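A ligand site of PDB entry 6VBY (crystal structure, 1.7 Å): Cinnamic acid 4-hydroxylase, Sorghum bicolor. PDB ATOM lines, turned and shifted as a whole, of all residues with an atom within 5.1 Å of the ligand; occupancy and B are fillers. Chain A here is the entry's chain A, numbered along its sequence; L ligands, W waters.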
ATOM      1  N   LEU A  91      -1.566  -2.172 -21.987  1.00  0.00           N
ATOM      2  CA  LEU A  91      -2.551  -3.066 -21.386  1.00  0.00           C
ATOM      3  C   LEU A  91      -1.942  -4.005 -20.366  1.00  0.00           C
ATOM      4  O   LEU A  91      -2.640  -4.419 -19.421  1.00  0.00           O
ATOM      5  CB  LEU A  91      -3.240  -3.883 -22.476  1.00  0.00           C
ATOM      6  CG  LEU A  91      -3.847  -3.088 -23.640  1.00  0.00           C
ATOM      7  CD1 LEU A  91      -4.365  -4.036 -24.717  1.00  0.00           C
ATOM      8  CD2 LEU A  91      -4.962  -2.179 -23.149  1.00  0.00           C
ATOM      9  N   ARG A 101      -9.490   5.143 -16.572  1.00  0.00           N
ATOM     10  CA  ARG A 101     -10.352   5.614 -17.635  1.00  0.00           C
ATOM     11  C   ARG A 101     -10.320   7.135 -17.666  1.00  0.00           C
ATOM     12  O   ARG A 101     -10.139   7.778 -16.633  1.00  0.00           O
ATOM     13  CB  ARG A 101     -11.794   5.135 -17.447  1.00  0.00           C
ATOM     14  CG  ARG A 101     -11.953   3.655 -17.168  1.00  0.00           C
ATOM     15  CD  ARG A 101     -11.293   2.871 -18.276  1.00  0.00           C
ATOM     16  NE  ARG A 101     -11.779   1.504 -18.396  1.00  0.00           N
ATOM     17  CZ  ARG A 101     -11.382   0.688 -19.371  1.00  0.00           C
ATOM     18  NH1 ARG A 101     -10.506   1.118 -20.267  1.00  0.00           N
ATOM     19  NH2 ARG A 101     -11.850  -0.556 -19.438  1.00  0.00           N
ATOM     20  N   MET A 117     -18.235   0.716 -12.616  1.00  0.00           N
ATOM     21  CA  MET A 117     -17.190  -0.268 -12.871  1.00  0.00           C
ATOM     22  C   MET A 117     -16.341   0.093 -14.076  1.00  0.00           C
ATOM     23  O   MET A 117     -15.101   0.031 -14.008  1.00  0.00           O
ATOM     24  CB  MET A 117     -17.838  -1.651 -13.085  1.00  0.00           C
ATOM     25  CG  MET A 117     -16.897  -2.736 -13.565  1.00  0.00           C
ATOM     26  SD  MET A 117     -16.082  -3.596 -12.208  1.00  0.00           S
ATOM     27  CE  MET A 117     -14.535  -2.715 -12.132  1.00  0.00           C
ATOM     28  N   VAL A 118     -16.971   0.456 -15.181  1.00  0.00           N
ATOM     29  CA  VAL A 118     -16.223   0.665 -16.418  1.00  0.00           C
ATOM     30  C   VAL A 118     -15.366   1.918 -16.332  1.00  0.00           C
ATOM     31  O   VAL A 118     -14.169   1.890 -16.620  1.00  0.00           O
ATOM     32  CB  VAL A 118     -17.175   0.723 -17.625  1.00  0.00           C
ATOM     33  CG1 VAL A 118     -16.420   1.138 -18.867  1.00  0.00           C
ATOM     34  CG2 VAL A 118     -17.856  -0.615 -17.814  1.00  0.00           C
ATOM     35  N   TRP A 126     -12.158   0.347  -7.924  1.00  0.00           N
ATOM     36  CA  TRP A 126     -12.225  -0.522  -9.081  1.00  0.00           C
ATOM     37  C   TRP A 126     -11.963  -1.970  -8.697  1.00  0.00           C
ATOM     38  O   TRP A 126     -12.660  -2.882  -9.164  1.00  0.00           O
ATOM     39  CB  TRP A 126     -11.226  -0.061 -10.140  1.00  0.00           C
ATOM     40  CG  TRP A 126     -11.091  -1.051 -11.250  1.00  0.00           C
ATOM     41  CD1 TRP A 126     -11.864  -1.128 -12.366  1.00  0.00           C
ATOM     42  CD2 TRP A 126     -10.141  -2.114 -11.330  1.00  0.00           C
ATOM     43  NE1 TRP A 126     -11.455  -2.183 -13.142  1.00  0.00           N
ATOM     44  CE2 TRP A 126     -10.396  -2.805 -12.534  1.00  0.00           C
ATOM     45  CE3 TRP A 126      -9.102  -2.551 -10.510  1.00  0.00           C
ATOM     46  CZ2 TRP A 126      -9.656  -3.899 -12.936  1.00  0.00           C
ATOM     47  CZ3 TRP A 126      -8.361  -3.644 -10.912  1.00  0.00           C
ATOM     48  CH2 TRP A 126      -8.637  -4.305 -12.116  1.00  0.00           C
ATOM     49  N   ARG A 130     -14.724  -4.842  -9.376  1.00  0.00           N
ATOM     50  CA  ARG A 130     -14.341  -5.966 -10.216  1.00  0.00           C
ATOM     51  C   ARG A 130     -14.490  -7.281  -9.465  1.00  0.00           C
ATOM     52  O   ARG A 130     -14.944  -8.281 -10.024  1.00  0.00           O
ATOM     53  CB  ARG A 130     -12.902  -5.790 -10.710  1.00  0.00           C
ATOM     54  CG  ARG A 130     -12.420  -6.840 -11.697  1.00  0.00           C
ATOM     55  CD  ARG A 130     -12.582  -6.388 -13.143  1.00  0.00           C
ATOM     56  NE  ARG A 130     -11.944  -7.317 -14.083  1.00  0.00           N
ATOM     57  CZ  ARG A 130     -11.726  -7.051 -15.366  1.00  0.00           C
ATOM     58  NH1 ARG A 130     -12.088  -5.886 -15.888  1.00  0.00           N
ATOM     59  NH2 ARG A 130     -11.130  -7.966 -16.139  1.00  0.00           N
ATOM     60  N   MET A 133     -18.271  -8.352  -8.800  1.00  0.00           N
ATOM     61  CA  MET A 133     -18.989  -8.751  -9.995  1.00  0.00           C
ATOM     62  C   MET A 133     -18.554 -10.115 -10.533  1.00  0.00           C
ATOM     63  O   MET A 133     -19.257 -10.686 -11.366  1.00  0.00           O
ATOM     64  CB  MET A 133     -18.812  -7.685 -11.085  1.00  0.00           C
ATOM     65  CG  MET A 133     -19.542  -6.388 -10.783  1.00  0.00           C
ATOM     66  SD  MET A 133     -19.400  -5.146 -12.093  1.00  0.00           S
ATOM     67  CE  MET A 133     -20.228  -5.994 -13.436  1.00  0.00           C
ATOM     68  N   PHE A 138     -19.353 -13.525 -14.070  1.00  0.00           N
ATOM     69  CA  PHE A 138     -18.216 -13.795 -14.943  1.00  0.00           C
ATOM     70  C   PHE A 138     -17.475 -15.060 -14.548  1.00  0.00           C
ATOM     71  O   PHE A 138     -16.246 -15.061 -14.389  1.00  0.00           O
ATOM     72  CB  PHE A 138     -17.285 -12.600 -14.942  1.00  0.00           C
ATOM     73  CG  PHE A 138     -17.934 -11.302 -15.359  1.00  0.00           C
ATOM     74  CD1 PHE A 138     -18.612 -11.207 -16.557  1.00  0.00           C
ATOM     75  CD2 PHE A 138     -17.840 -10.160 -14.555  1.00  0.00           C
ATOM     76  CE1 PHE A 138     -19.194 -10.012 -16.956  1.00  0.00           C
ATOM     77  CE2 PHE A 138     -18.410  -8.970 -14.949  1.00  0.00           C
ATOM     78  CZ  PHE A 138     -19.093  -8.891 -16.148  1.00  0.00           C
ATOM     79  N   MET A 186     -29.159 -10.802 -21.314  1.00  0.00           N
ATOM     80  CA  MET A 186     -28.515 -10.052 -20.257  1.00  0.00           C
ATOM     81  C   MET A 186     -29.433  -9.815 -19.066  1.00  0.00           C
ATOM     82  O   MET A 186     -28.964  -9.798 -17.923  1.00  0.00           O
ATOM     83  CB  MET A 186     -27.992  -8.725 -20.799  1.00  0.00           C
ATOM     84  CG  MET A 186     -26.869  -8.890 -21.806  1.00  0.00           C
ATOM     85  SD  MET A 186     -25.500  -9.866 -21.137  1.00  0.00           S
ATOM     86  CE  MET A 186     -24.588 -10.266 -22.620  1.00  0.00           C
ATOM     87  N   ILE A 299     -23.770  -2.452 -17.341  1.00  0.00           N
ATOM     88  CA  ILE A 299     -24.057  -3.642 -18.126  1.00  0.00           C
ATOM     89  C   ILE A 299     -24.932  -3.299 -19.323  1.00  0.00           C
ATOM     90  O   ILE A 299     -24.774  -3.864 -20.414  1.00  0.00           O
ATOM     91  CB  ILE A 299     -24.700  -4.728 -17.241  1.00  0.00           C
ATOM     92  CG1 ILE A 299     -23.662  -5.239 -16.238  1.00  0.00           C
ATOM     93  CG2 ILE A 299     -25.232  -5.867 -18.092  1.00  0.00           C
ATOM     94  CD1 ILE A 299     -24.260  -5.886 -15.025  1.00  0.00           C
ATOM     95  N   ALA A 302     -22.570  -1.796 -21.873  1.00  0.00           N
ATOM     96  CA  ALA A 302     -21.362  -2.553 -22.189  1.00  0.00           C
ATOM     97  C   ALA A 302     -21.624  -3.886 -22.861  1.00  0.00           C
ATOM     98  O   ALA A 302     -20.734  -4.409 -23.522  1.00  0.00           O
ATOM     99  CB  ALA A 302     -20.547  -2.787 -20.916  1.00  0.00           C
ATOM    100  N   ALA A 303     -22.824  -4.441 -22.712  1.00  0.00           N
ATOM    101  CA  ALA A 303     -23.034  -5.857 -22.994  1.00  0.00           C
ATOM    102  C   ALA A 303     -24.023  -6.145 -24.105  1.00  0.00           C
ATOM    103  O   ALA A 303     -23.927  -7.203 -24.735  1.00  0.00           O
ATOM    104  CB  ALA A 303     -23.518  -6.577 -21.729  1.00  0.00           C
ATOM    105  N   THR A 306     -23.232  -4.123 -27.915  1.00  0.00           N
ATOM    106  CA  THR A 306     -21.867  -4.494 -28.265  1.00  0.00           C
ATOM    107  C   THR A 306     -21.810  -5.906 -28.843  1.00  0.00           C
ATOM    108  O   THR A 306     -21.217  -6.142 -29.895  1.00  0.00           O
ATOM    109  CB  THR A 306     -20.979  -4.381 -27.037  1.00  0.00           C
ATOM    110  OG1 THR A 306     -21.546  -5.168 -25.980  1.00  0.00           O
ATOM    111  CG2 THR A 306     -20.890  -2.932 -26.574  1.00  0.00           C
ATOM    112  N   THR A 307     -22.427  -6.865 -28.138  1.00  0.00           N
ATOM    113  CA  THR A 307     -22.484  -8.229 -28.642  1.00  0.00           C
ATOM    114  C   THR A 307     -23.303  -8.279 -29.928  1.00  0.00           C
ATOM    115  O   THR A 307     -22.958  -9.021 -30.864  1.00  0.00           O
ATOM    116  CB  THR A 307     -23.092  -9.149 -27.585  1.00  0.00           C
ATOM    117  OG1 THR A 307     -22.430  -8.951 -26.334  1.00  0.00           O
ATOM    118  CG2 THR A 307     -22.943 -10.608 -28.010  1.00  0.00           C
ATOM    119  N   SER A 310     -21.397  -7.607 -33.250  1.00  0.00           N
ATOM    120  CA  SER A 310     -20.614  -8.729 -33.749  1.00  0.00           C
ATOM    121  C   SER A 310     -21.505  -9.799 -34.365  1.00  0.00           C
ATOM    122  O   SER A 310     -21.158 -10.378 -35.399  1.00  0.00           O
ATOM    123  CB  SER A 310     -19.769  -9.325 -32.616  1.00  0.00           C
ATOM    124  OG  SER A 310     -18.760  -8.418 -32.215  1.00  0.00           O
ATOM    125  N   LEU A 361     -14.751 -10.999 -35.039  1.00  0.00           N
ATOM    126  CA  LEU A 361     -14.145 -10.065 -34.100  1.00  0.00           C
ATOM    127  C   LEU A 361     -12.863  -9.453 -34.642  1.00  0.00           C
ATOM    128  O   LEU A 361     -12.475  -8.377 -34.192  1.00  0.00           O
ATOM    129  CB  LEU A 361     -13.857 -10.778 -32.776  1.00  0.00           C
ATOM    130  CG  LEU A 361     -15.054 -11.287 -31.978  1.00  0.00           C
ATOM    131  CD1 LEU A 361     -14.614 -12.319 -30.941  1.00  0.00           C
ATOM    132  CD2 LEU A 361     -15.769 -10.132 -31.310  1.00  0.00           C
ATOM    133  N   ILE A 367     -15.757  -2.917 -31.441  1.00  0.00           N
ATOM    134  CA  ILE A 367     -15.244  -1.948 -30.477  1.00  0.00           C
ATOM    135  C   ILE A 367     -13.790  -1.696 -30.874  1.00  0.00           C
ATOM    136  O   ILE A 367     -12.870  -2.238 -30.242  1.00  0.00           O
ATOM    137  CB  ILE A 367     -15.394  -2.444 -29.029  1.00  0.00           C
ATOM    138  CG1 ILE A 367     -16.873  -2.794 -28.788  1.00  0.00           C
ATOM    139  CG2 ILE A 367     -14.957  -1.372 -28.060  1.00  0.00           C
ATOM    140  CD1 ILE A 367     -17.206  -3.195 -27.379  1.00  0.00           C
ATOM    141  N   LEU A 370     -11.074  -0.180 -28.453  1.00  0.00           N
ATOM    142  CA  LEU A 370     -11.299  -0.666 -27.095  1.00  0.00           C
ATOM    143  C   LEU A 370     -12.081   0.375 -26.298  1.00  0.00           C
ATOM    144  O   LEU A 370     -13.053   0.951 -26.802  1.00  0.00           O
ATOM    145  CB  LEU A 370      -9.960  -0.996 -26.431  1.00  0.00           C
ATOM    146  CG  LEU A 370      -9.012  -1.902 -27.238  1.00  0.00           C
ATOM    147  CD1 LEU A 370      -7.814  -2.301 -26.399  1.00  0.00           C
ATOM    148  CD2 LEU A 370      -9.749  -3.130 -27.763  1.00  0.00           C
ATOM    149  N   VAL A 371     -11.680   0.593 -25.057  1.00  0.00           N
ATOM    150  CA  VAL A 371     -12.217   1.644 -24.199  1.00  0.00           C
ATOM    151  C   VAL A 371     -11.022   2.541 -23.876  1.00  0.00           C
ATOM    152  O   VAL A 371      -9.897   2.030 -23.773  1.00  0.00           O
ATOM    153  CB  VAL A 371     -12.877   1.074 -22.937  1.00  0.00           C
ATOM    154  CG1 VAL A 371     -13.230   2.175 -21.967  1.00  0.00           C
ATOM    155  CG2 VAL A 371     -14.118   0.272 -23.318  1.00  0.00           C
ATOM    156  N   HIS A 373      -8.013   4.277 -22.199  1.00  0.00           N
ATOM    157  CA  HIS A 373      -7.194   4.167 -21.010  1.00  0.00           C
ATOM    158  C   HIS A 373      -6.667   5.547 -20.627  1.00  0.00           C
ATOM    159  O   HIS A 373      -6.774   6.507 -21.390  1.00  0.00           O
ATOM    160  CB  HIS A 373      -6.059   3.174 -21.235  1.00  0.00           C
ATOM    161  CG  HIS A 373      -6.488   1.737 -21.215  1.00  0.00           C
ATOM    162  ND1 HIS A 373      -5.993   0.823 -20.312  1.00  0.00           N
ATOM    163  CD2 HIS A 373      -7.385   1.069 -21.971  1.00  0.00           C
ATOM    164  CE1 HIS A 373      -6.559  -0.355 -20.521  1.00  0.00           C
ATOM    165  NE2 HIS A 373      -7.409  -0.229 -21.530  1.00  0.00           N
ATOM    166  N   VAL A 434      -6.710  -8.274 -29.860  1.00  0.00           N
ATOM    167  CA  VAL A 434      -7.135  -7.979 -28.499  1.00  0.00           C
ATOM    168  C   VAL A 434      -8.558  -7.430 -28.496  1.00  0.00           C
ATOM    169  O   VAL A 434      -8.820  -6.388 -27.887  1.00  0.00           O
ATOM    170  CB  VAL A 434      -6.164  -7.005 -27.807  1.00  0.00           C
ATOM    171  CG1 VAL A 434      -4.816  -7.678 -27.566  1.00  0.00           C
ATOM    172  CG2 VAL A 434      -5.977  -5.732 -28.635  1.00  0.00           C
ATOM    173  N   PRO A 435      -9.511  -8.118 -29.124  1.00  0.00           N
ATOM    174  CA  PRO A 435     -10.885  -7.577 -29.194  1.00  0.00           C
ATOM    175  C   PRO A 435     -11.531  -7.386 -27.839  1.00  0.00           C
ATOM    176  O   PRO A 435     -12.454  -6.556 -27.719  1.00  0.00           O
ATOM    177  CB  PRO A 435     -11.636  -8.621 -30.028  1.00  0.00           C
ATOM    178  CG  PRO A 435     -10.842  -9.907 -29.832  1.00  0.00           C
ATOM    179  CD  PRO A 435      -9.407  -9.456 -29.734  1.00  0.00           C
ATOM    180  N   PHE A 436     -11.104  -8.119 -26.812  1.00  0.00           N
ATOM    181  CA  PHE A 436     -11.616  -7.984 -25.463  1.00  0.00           C
ATOM    182  C   PHE A 436     -10.584  -7.387 -24.520  1.00  0.00           C
ATOM    183  O   PHE A 436     -10.705  -7.514 -23.295  1.00  0.00           O
ATOM    184  CB  PHE A 436     -12.089  -9.334 -24.924  1.00  0.00           C
ATOM    185  CG  PHE A 436     -13.296  -9.880 -25.632  1.00  0.00           C
ATOM    186  CD1 PHE A 436     -14.566  -9.527 -25.233  1.00  0.00           C
ATOM    187  CD2 PHE A 436     -13.148 -10.763 -26.691  1.00  0.00           C
ATOM    188  CE1 PHE A 436     -15.676 -10.027 -25.876  1.00  0.00           C
ATOM    189  CE2 PHE A 436     -14.257 -11.269 -27.342  1.00  0.00           C
ATOM    190  CZ  PHE A 436     -15.519 -10.907 -26.935  1.00  0.00           C
ATOM    191  N   GLY A 437      -9.571  -6.728 -25.067  1.00  0.00           N
ATOM    192  CA  GLY A 437      -8.514  -6.211 -24.249  1.00  0.00           C
ATOM    193  C   GLY A 437      -7.622  -7.306 -23.683  1.00  0.00           C
ATOM    194  O   GLY A 437      -7.750  -8.495 -23.998  1.00  0.00           O
ATOM    195  N   VAL A 438      -6.693  -6.871 -22.837  1.00  0.00           N
ATOM    196  CA  VAL A 438      -5.761  -7.765 -22.159  1.00  0.00           C
ATOM    197  C   VAL A 438      -5.505  -7.190 -20.778  1.00  0.00           C
ATOM    198  O   VAL A 438      -5.480  -5.978 -20.589  1.00  0.00           O
ATOM    199  CB  VAL A 438      -4.424  -7.937 -22.915  1.00  0.00           C
ATOM    200  CG1 VAL A 438      -3.516  -8.898 -22.158  1.00  0.00           C
ATOM    201  CG2 VAL A 438      -4.656  -8.405 -24.341  1.00  0.00           C
ATOM    202  N   ARG A 440      -5.510  -6.064 -16.827  1.00  0.00           N
ATOM    203  CA  ARG A 440      -6.317  -5.689 -15.667  1.00  0.00           C
ATOM    204  C   ARG A 440      -7.669  -5.118 -16.082  1.00  0.00           C
ATOM    205  O   ARG A 440      -8.691  -5.435 -15.452  1.00  0.00           O
ATOM    206  CB  ARG A 440      -5.538  -4.693 -14.808  1.00  0.00           C
ATOM    207  CG  ARG A 440      -4.362  -5.314 -14.065  1.00  0.00           C
ATOM    208  CD  ARG A 440      -3.489  -4.247 -13.425  1.00  0.00           C
ATOM    209  NE  ARG A 440      -2.426  -4.816 -12.585  1.00  0.00           N
ATOM    210  CZ  ARG A 440      -1.267  -5.270 -13.064  1.00  0.00           C
ATOM    211  NH1 ARG A 440      -1.025  -5.241 -14.365  1.00  0.00           N
ATOM    212  NH2 ARG A 440      -0.357  -5.758 -12.227  1.00  0.00           N
ATOM    213  N   ARG A 441      -7.719  -4.277 -17.109  1.00  0.00           N
ATOM    214  CA  ARG A 441      -8.971  -3.660 -17.531  1.00  0.00           C
ATOM    215  C   ARG A 441      -9.632  -4.419 -18.681  1.00  0.00           C
ATOM    216  O   ARG A 441     -10.490  -3.849 -19.361  1.00  0.00           O
ATOM    217  CB  ARG A 441      -8.764  -2.200 -17.936  1.00  0.00           C
ATOM    218  CG  ARG A 441      -8.202  -1.258 -16.875  1.00  0.00           C
ATOM    219  CD  ARG A 441      -8.972  -1.284 -15.571  1.00  0.00           C
ATOM    220  NE  ARG A 441     -10.353  -0.815 -15.630  1.00  0.00           N
ATOM    221  CZ  ARG A 441     -10.781   0.350 -15.138  1.00  0.00           C
ATOM    222  NH1 ARG A 441      -9.942   1.210 -14.568  1.00  0.00           N
ATOM    223  NH2 ARG A 441     -12.069   0.656 -15.220  1.00  0.00           N
ATOM    224  N   SER A 442      -9.247  -5.670 -18.913  1.00  0.00           N
ATOM    225  CA  SER A 442      -9.817  -6.434 -20.011  1.00  0.00           C
ATOM    226  C   SER A 442     -11.295  -6.723 -19.775  1.00  0.00           C
ATOM    227  O   SER A 442     -11.809  -6.612 -18.653  1.00  0.00           O
ATOM    228  CB  SER A 442      -9.068  -7.756 -20.197  1.00  0.00           C
ATOM    229  OG  SER A 442      -9.230  -8.598 -19.075  1.00  0.00           O
ATOM    230  N   CYS A 443     -11.975  -7.105 -20.843  1.00  0.00           N
ATOM    231  CA  CYS A 443     -13.406  -7.383 -20.742  1.00  0.00           C
ATOM    232  C   CYS A 443     -13.644  -8.623 -19.894  1.00  0.00           C
ATOM    233  O   CYS A 443     -13.198  -9.719 -20.284  1.00  0.00           O
ATOM    234  CB  CYS A 443     -14.008  -7.574 -22.123  1.00  0.00           C
ATOM    235  SG  CYS A 443     -15.751  -8.039 -22.057  1.00  0.00           S
ATOM    236  N   PRO A 444     -14.343  -8.525 -18.762  1.00  0.00           N
ATOM    237  CA  PRO A 444     -14.760  -9.741 -18.052  1.00  0.00           C
ATOM    238  C   PRO A 444     -15.902 -10.450 -18.751  1.00  0.00           C
ATOM    239  O   PRO A 444     -16.096 -11.645 -18.524  1.00  0.00           O
ATOM    240  CB  PRO A 444     -15.169  -9.228 -16.666  1.00  0.00           C
ATOM    241  CG  PRO A 444     -15.695  -7.850 -16.952  1.00  0.00           C
ATOM    242  CD  PRO A 444     -14.881  -7.304 -18.117  1.00  0.00           C
ATOM    243  N   GLY A 445     -16.650  -9.746 -19.592  1.00  0.00           N
ATOM    244  CA  GLY A 445     -17.789 -10.335 -20.287  1.00  0.00           C
ATOM    245  C   GLY A 445     -17.428 -11.249 -21.432  1.00  0.00           C
ATOM    246  O   GLY A 445     -18.338 -11.863 -22.019  1.00  0.00           O
ATOM    247  N   LEU A 448     -19.084 -14.486 -21.478  1.00  0.00           N
ATOM    248  CA  LEU A 448     -20.481 -14.525 -21.886  1.00  0.00           C
ATOM    249  C   LEU A 448     -20.660 -14.227 -23.376  1.00  0.00           C
ATOM    250  O   LEU A 448     -21.496 -14.860 -24.026  1.00  0.00           O
ATOM    251  CB  LEU A 448     -21.295 -13.511 -21.075  1.00  0.00           C
ATOM    252  CG  LEU A 448     -21.066 -13.498 -19.559  1.00  0.00           C
ATOM    253  CD1 LEU A 448     -21.827 -12.341 -18.935  1.00  0.00           C
ATOM    254  CD2 LEU A 448     -21.466 -14.820 -18.933  1.00  0.00           C
ATOM    255  N   ALA A 449     -19.895 -13.287 -23.903  1.00  0.00           N
ATOM    256  CA  ALA A 449     -20.097 -12.859 -25.289  1.00  0.00           C
ATOM    257  C   ALA A 449     -19.759 -13.979 -26.260  1.00  0.00           C
ATOM    258  O   ALA A 449     -20.497 -14.219 -27.225  1.00  0.00           O
ATOM    259  CB  ALA A 449     -19.238 -11.620 -25.582  1.00  0.00           C
ATOM    260  N   ILE A 453     -22.478 -15.357 -29.042  1.00  0.00           N
ATOM    261  CA  ILE A 453     -22.292 -15.161 -30.475  1.00  0.00           C
ATOM    262  C   ILE A 453     -22.283 -16.500 -31.195  1.00  0.00           C
ATOM    263  O   ILE A 453     -22.951 -16.682 -32.226  1.00  0.00           O
ATOM    264  CB  ILE A 453     -21.015 -14.367 -30.765  1.00  0.00           C
ATOM    265  CG1 ILE A 453     -21.097 -12.963 -30.148  1.00  0.00           C
ATOM    266  CG2 ILE A 453     -20.788 -14.287 -32.272  1.00  0.00           C
ATOM    267  CD1 ILE A 453     -19.741 -12.276 -30.075  1.00  0.00           C
HETATM  268  C1  LIG L   1     -14.660  -3.769 -21.059  1.00  0.00           C
HETATM  269  C2  LIG L   1     -15.069  -5.704 -25.486  1.00  0.00           C
HETATM  270  C3  LIG L   1     -19.249  -7.766 -24.152  1.00  0.00           C
HETATM  271  C4  LIG L   1     -18.637  -6.108 -19.643  1.00  0.00           C
HETATM  272  C5  LIG L   1     -14.434  -4.088 -22.381  1.00  0.00           C
HETATM  273  C6  LIG L   1     -13.332  -3.610 -23.171  1.00  0.00           C
HETATM  274  C7  LIG L   1     -13.443  -4.133 -24.399  1.00  0.00           C
HETATM  275  C8  LIG L   1     -14.616  -4.978 -24.413  1.00  0.00           C
HETATM  276  C9  LIG L   1     -12.500  -3.895 -25.593  1.00  0.00           C
HETATM  277  C10 LIG L   1     -12.254  -2.626 -22.667  1.00  0.00           C
HETATM  278  C11 LIG L   1     -10.863  -3.234 -22.768  1.00  0.00           C
HETATM  279  C12 LIG L   1      -9.878  -2.182 -22.334  1.00  0.00           C
HETATM  280  O1  LIG L   1      -8.666  -2.325 -22.628  1.00  0.00           O
HETATM  281  O2  LIG L   1     -10.307  -1.171 -21.714  1.00  0.00           O
HETATM  282  C13 LIG L   1     -16.257  -6.409 -25.514  1.00  0.00           C
HETATM  283  C14 LIG L   1     -16.820  -7.052 -26.681  1.00  0.00           C
HETATM  284  C15 LIG L   1     -17.976  -7.613 -26.316  1.00  0.00           C
HETATM  285  C16 LIG L   1     -18.179  -7.342 -24.909  1.00  0.00           C
HETATM  286  C17 LIG L   1     -16.145  -7.052 -28.077  1.00  0.00           C
HETATM  287  C18 LIG L   1     -18.957  -8.444 -27.179  1.00  0.00           C
HETATM  288  C19 LIG L   1     -18.597  -8.944 -28.360  1.00  0.00           C
HETATM  289  C20 LIG L   1     -19.418  -7.548 -22.802  1.00  0.00           C
HETATM  290  C21 LIG L   1     -20.447  -8.142 -21.960  1.00  0.00           C
HETATM  291  C22 LIG L   1     -20.272  -7.679 -20.708  1.00  0.00           C
HETATM  292  C23 LIG L   1     -19.139  -6.786 -20.731  1.00  0.00           C
HETATM  293  C24 LIG L   1     -21.504  -9.130 -22.483  1.00  0.00           C
HETATM  294  C25 LIG L   1     -21.046  -7.948 -19.398  1.00  0.00           C
HETATM  295  C26 LIG L   1     -22.027  -8.841 -19.331  1.00  0.00           C
HETATM  296  C27 LIG L   1     -17.528  -5.296 -19.639  1.00  0.00           C
HETATM  297  C28 LIG L   1     -17.053  -4.527 -18.519  1.00  0.00           C
HETATM  298  C29 LIG L   1     -15.948  -3.878 -18.915  1.00  0.00           C
HETATM  299  C30 LIG L   1     -15.698  -4.224 -20.288  1.00  0.00           C
HETATM  300  C31 LIG L   1     -17.705  -4.466 -17.125  1.00  0.00           C
HETATM  301  C32 LIG L   1     -15.082  -2.924 -18.053  1.00  0.00           C
HETATM  302  C33 LIG L   1     -13.867  -3.648 -17.490  1.00  0.00           C
HETATM  303  C34 LIG L   1     -13.049  -2.713 -16.646  1.00  0.00           C
HETATM  304  O3  LIG L   1     -12.913  -1.509 -17.008  1.00  0.00           O
HETATM  305  O4  LIG L   1     -12.510  -3.167 -15.599  1.00  0.00           O
HETATM  306  N1  LIG L   1     -15.197  -4.919 -23.167  1.00  0.00           N
HETATM  307  N2  LIG L   1     -17.111  -6.601 -24.448  1.00  0.00           N
HETATM  308  N3  LIG L   1     -18.639  -6.735 -22.014  1.00  0.00           N
HETATM  309  N4  LIG L   1     -16.687  -5.099 -20.709  1.00  0.00           N
HETATM  310 FE1  LIG L   1     -16.897  -5.883 -22.562  1.00  0.00          FE
HETATM  311  O   HOH W   1     -15.718  -6.042 -31.138  1.00  0.00           O
HETATM  312  O   HOH W   2      -7.567  -4.465 -21.666  1.00  0.00           O
HETATM  313  O   HOH W   3     -18.418  -6.363 -30.648  1.00  0.00           O
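Water W2 lies within hydrogen-bond range of O1 of the ligand (2.6 Å), O of Val 438 (2.8 Å) and N of Ser 442 (3.4 Å).
Water W3 lies within hydrogen-bond range of OG of Ser 310 and O of Thr 306.
The backbone carbonyl oxygen (O) of Arg 440 sits close to the guanidinium group (NH1) of Arg 130 (3.5 Å).
O of Met 117 lies within hydrogen-bond range of NH2 of Arg 441, 3.3 Å away.
N of Arg 130 is in hydrogen-bond range of SD of Met 117, 3.4 Å away.
The side-chain hydroxyl of Thr 306 is in hydrogen-bond range of the backbone carbonyl oxygen of Ala 302 (2.7 Å).
O of Ser 442 lies within hydrogen-bond range of NH1 of Arg 130, 2.9 Å away.
The backbone NH of Cys 443 lies within hydrogen-bond range of the backbone carbonyl oxygen of Phe 436, 2.8 Å away.
O of Ala 303 lies close to OG1 of Thr 306, at 3.4 Å.
The backbone carbonyl oxygen of Val 118 lies close to the guanidinium group of Arg 101 (3.0 Å).
NE1 of Trp 126 is in hydrogen-bond range of O4 of the ligand (2.8 Å).
A ring nitrogen (NE2) of His 373 sits at hydrogen-bond distance from an oxygen (O1) of the ligand (2.7 Å).
An oxygen (O3) of the ligand is in salt-bridge range of the guanidinium group of Arg 441 (2.9 Å).
NH1 of Arg 101 is in salt-bridge range of O2 of the ligand (2.7 Å).
The side-chain sulfur (SG) of Cys 443 is bound to an iron atom (FE1) of the ligand (2.5 Å).
NH1 of Arg 130 is in salt-bridge range of O4 of the ligand (2.8 Å).
N3 of the ligand sits close to O of Ala 302, 3.5 Å away.
Leu 91 touches the ligand (CD2 to O1, 3.7 Å).
CG2 of Val 118 touches C32 of the ligand (3.6 Å).
Phe 138 touches the ligand (CE1 to C25, 3.7 Å).
Met 186 touches the ligand (CE to C24, 3.3 Å).
Ala 303 touches the ligand.
Thr 306 touches the ligand.
OG1 of Thr 307 touches C18 of the ligand, 3.6 Å away.
OG of Ser 310 touches C19 of the ligand, 3.9 Å away.
Ile 367 touches the ligand (CD1 to C2, 3.8 Å).
Leu 370 touches the ligand.
Val 371 touches the ligand (CG2 to C10, 3.5 Å).
O of Pro 435 touches C9 of the ligand, at 3.4 Å.
CE1 of Phe 436 touches C14 of the ligand (3.3 Å).
O of Ser 442 touches C33 of the ligand, 3.8 Å away.
Pro 444 touches the ligand (CD to C28, 3.5 Å).
CA of Gly 445 touches C22 of the ligand, 3.7 Å away.
CD1 of Leu 448 touches C26 of the ligand, at 3.5 Å.
Ala 449 touches the ligand.
Ile 453 touches the ligand.
Hydrophobic or aromatic side chains that line the ligand: Leu 91, Val 118, Trp 126, Phe 138, Met 186, Ala 303, Ile 367, Leu 370, Val 371, His 373, Phe 436, Pro 444, Leu 448, Ala 449 and Ile 453.
26 residues have an atom within 4 Å of the ligand: Leu 91, Arg 101, Val 118, Trp 126, Arg 130, Phe 138, Met 186, Ala 302, Ala 303, Thr 306, Thr 307, Ser 310, Ile 367, Leu 370, Val 371, His 373, Pro 435, Phe 436, Arg 441, Ser 442, Cys 443, Pro 444, Gly 445, Leu 448, Ala 449 and Ile 453.
Along chain A the residues within 4 Å of the ligand span positions 91 to 453.
The nearest printed residue that does not touch the ligand is Met 117 (4.02 Å).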
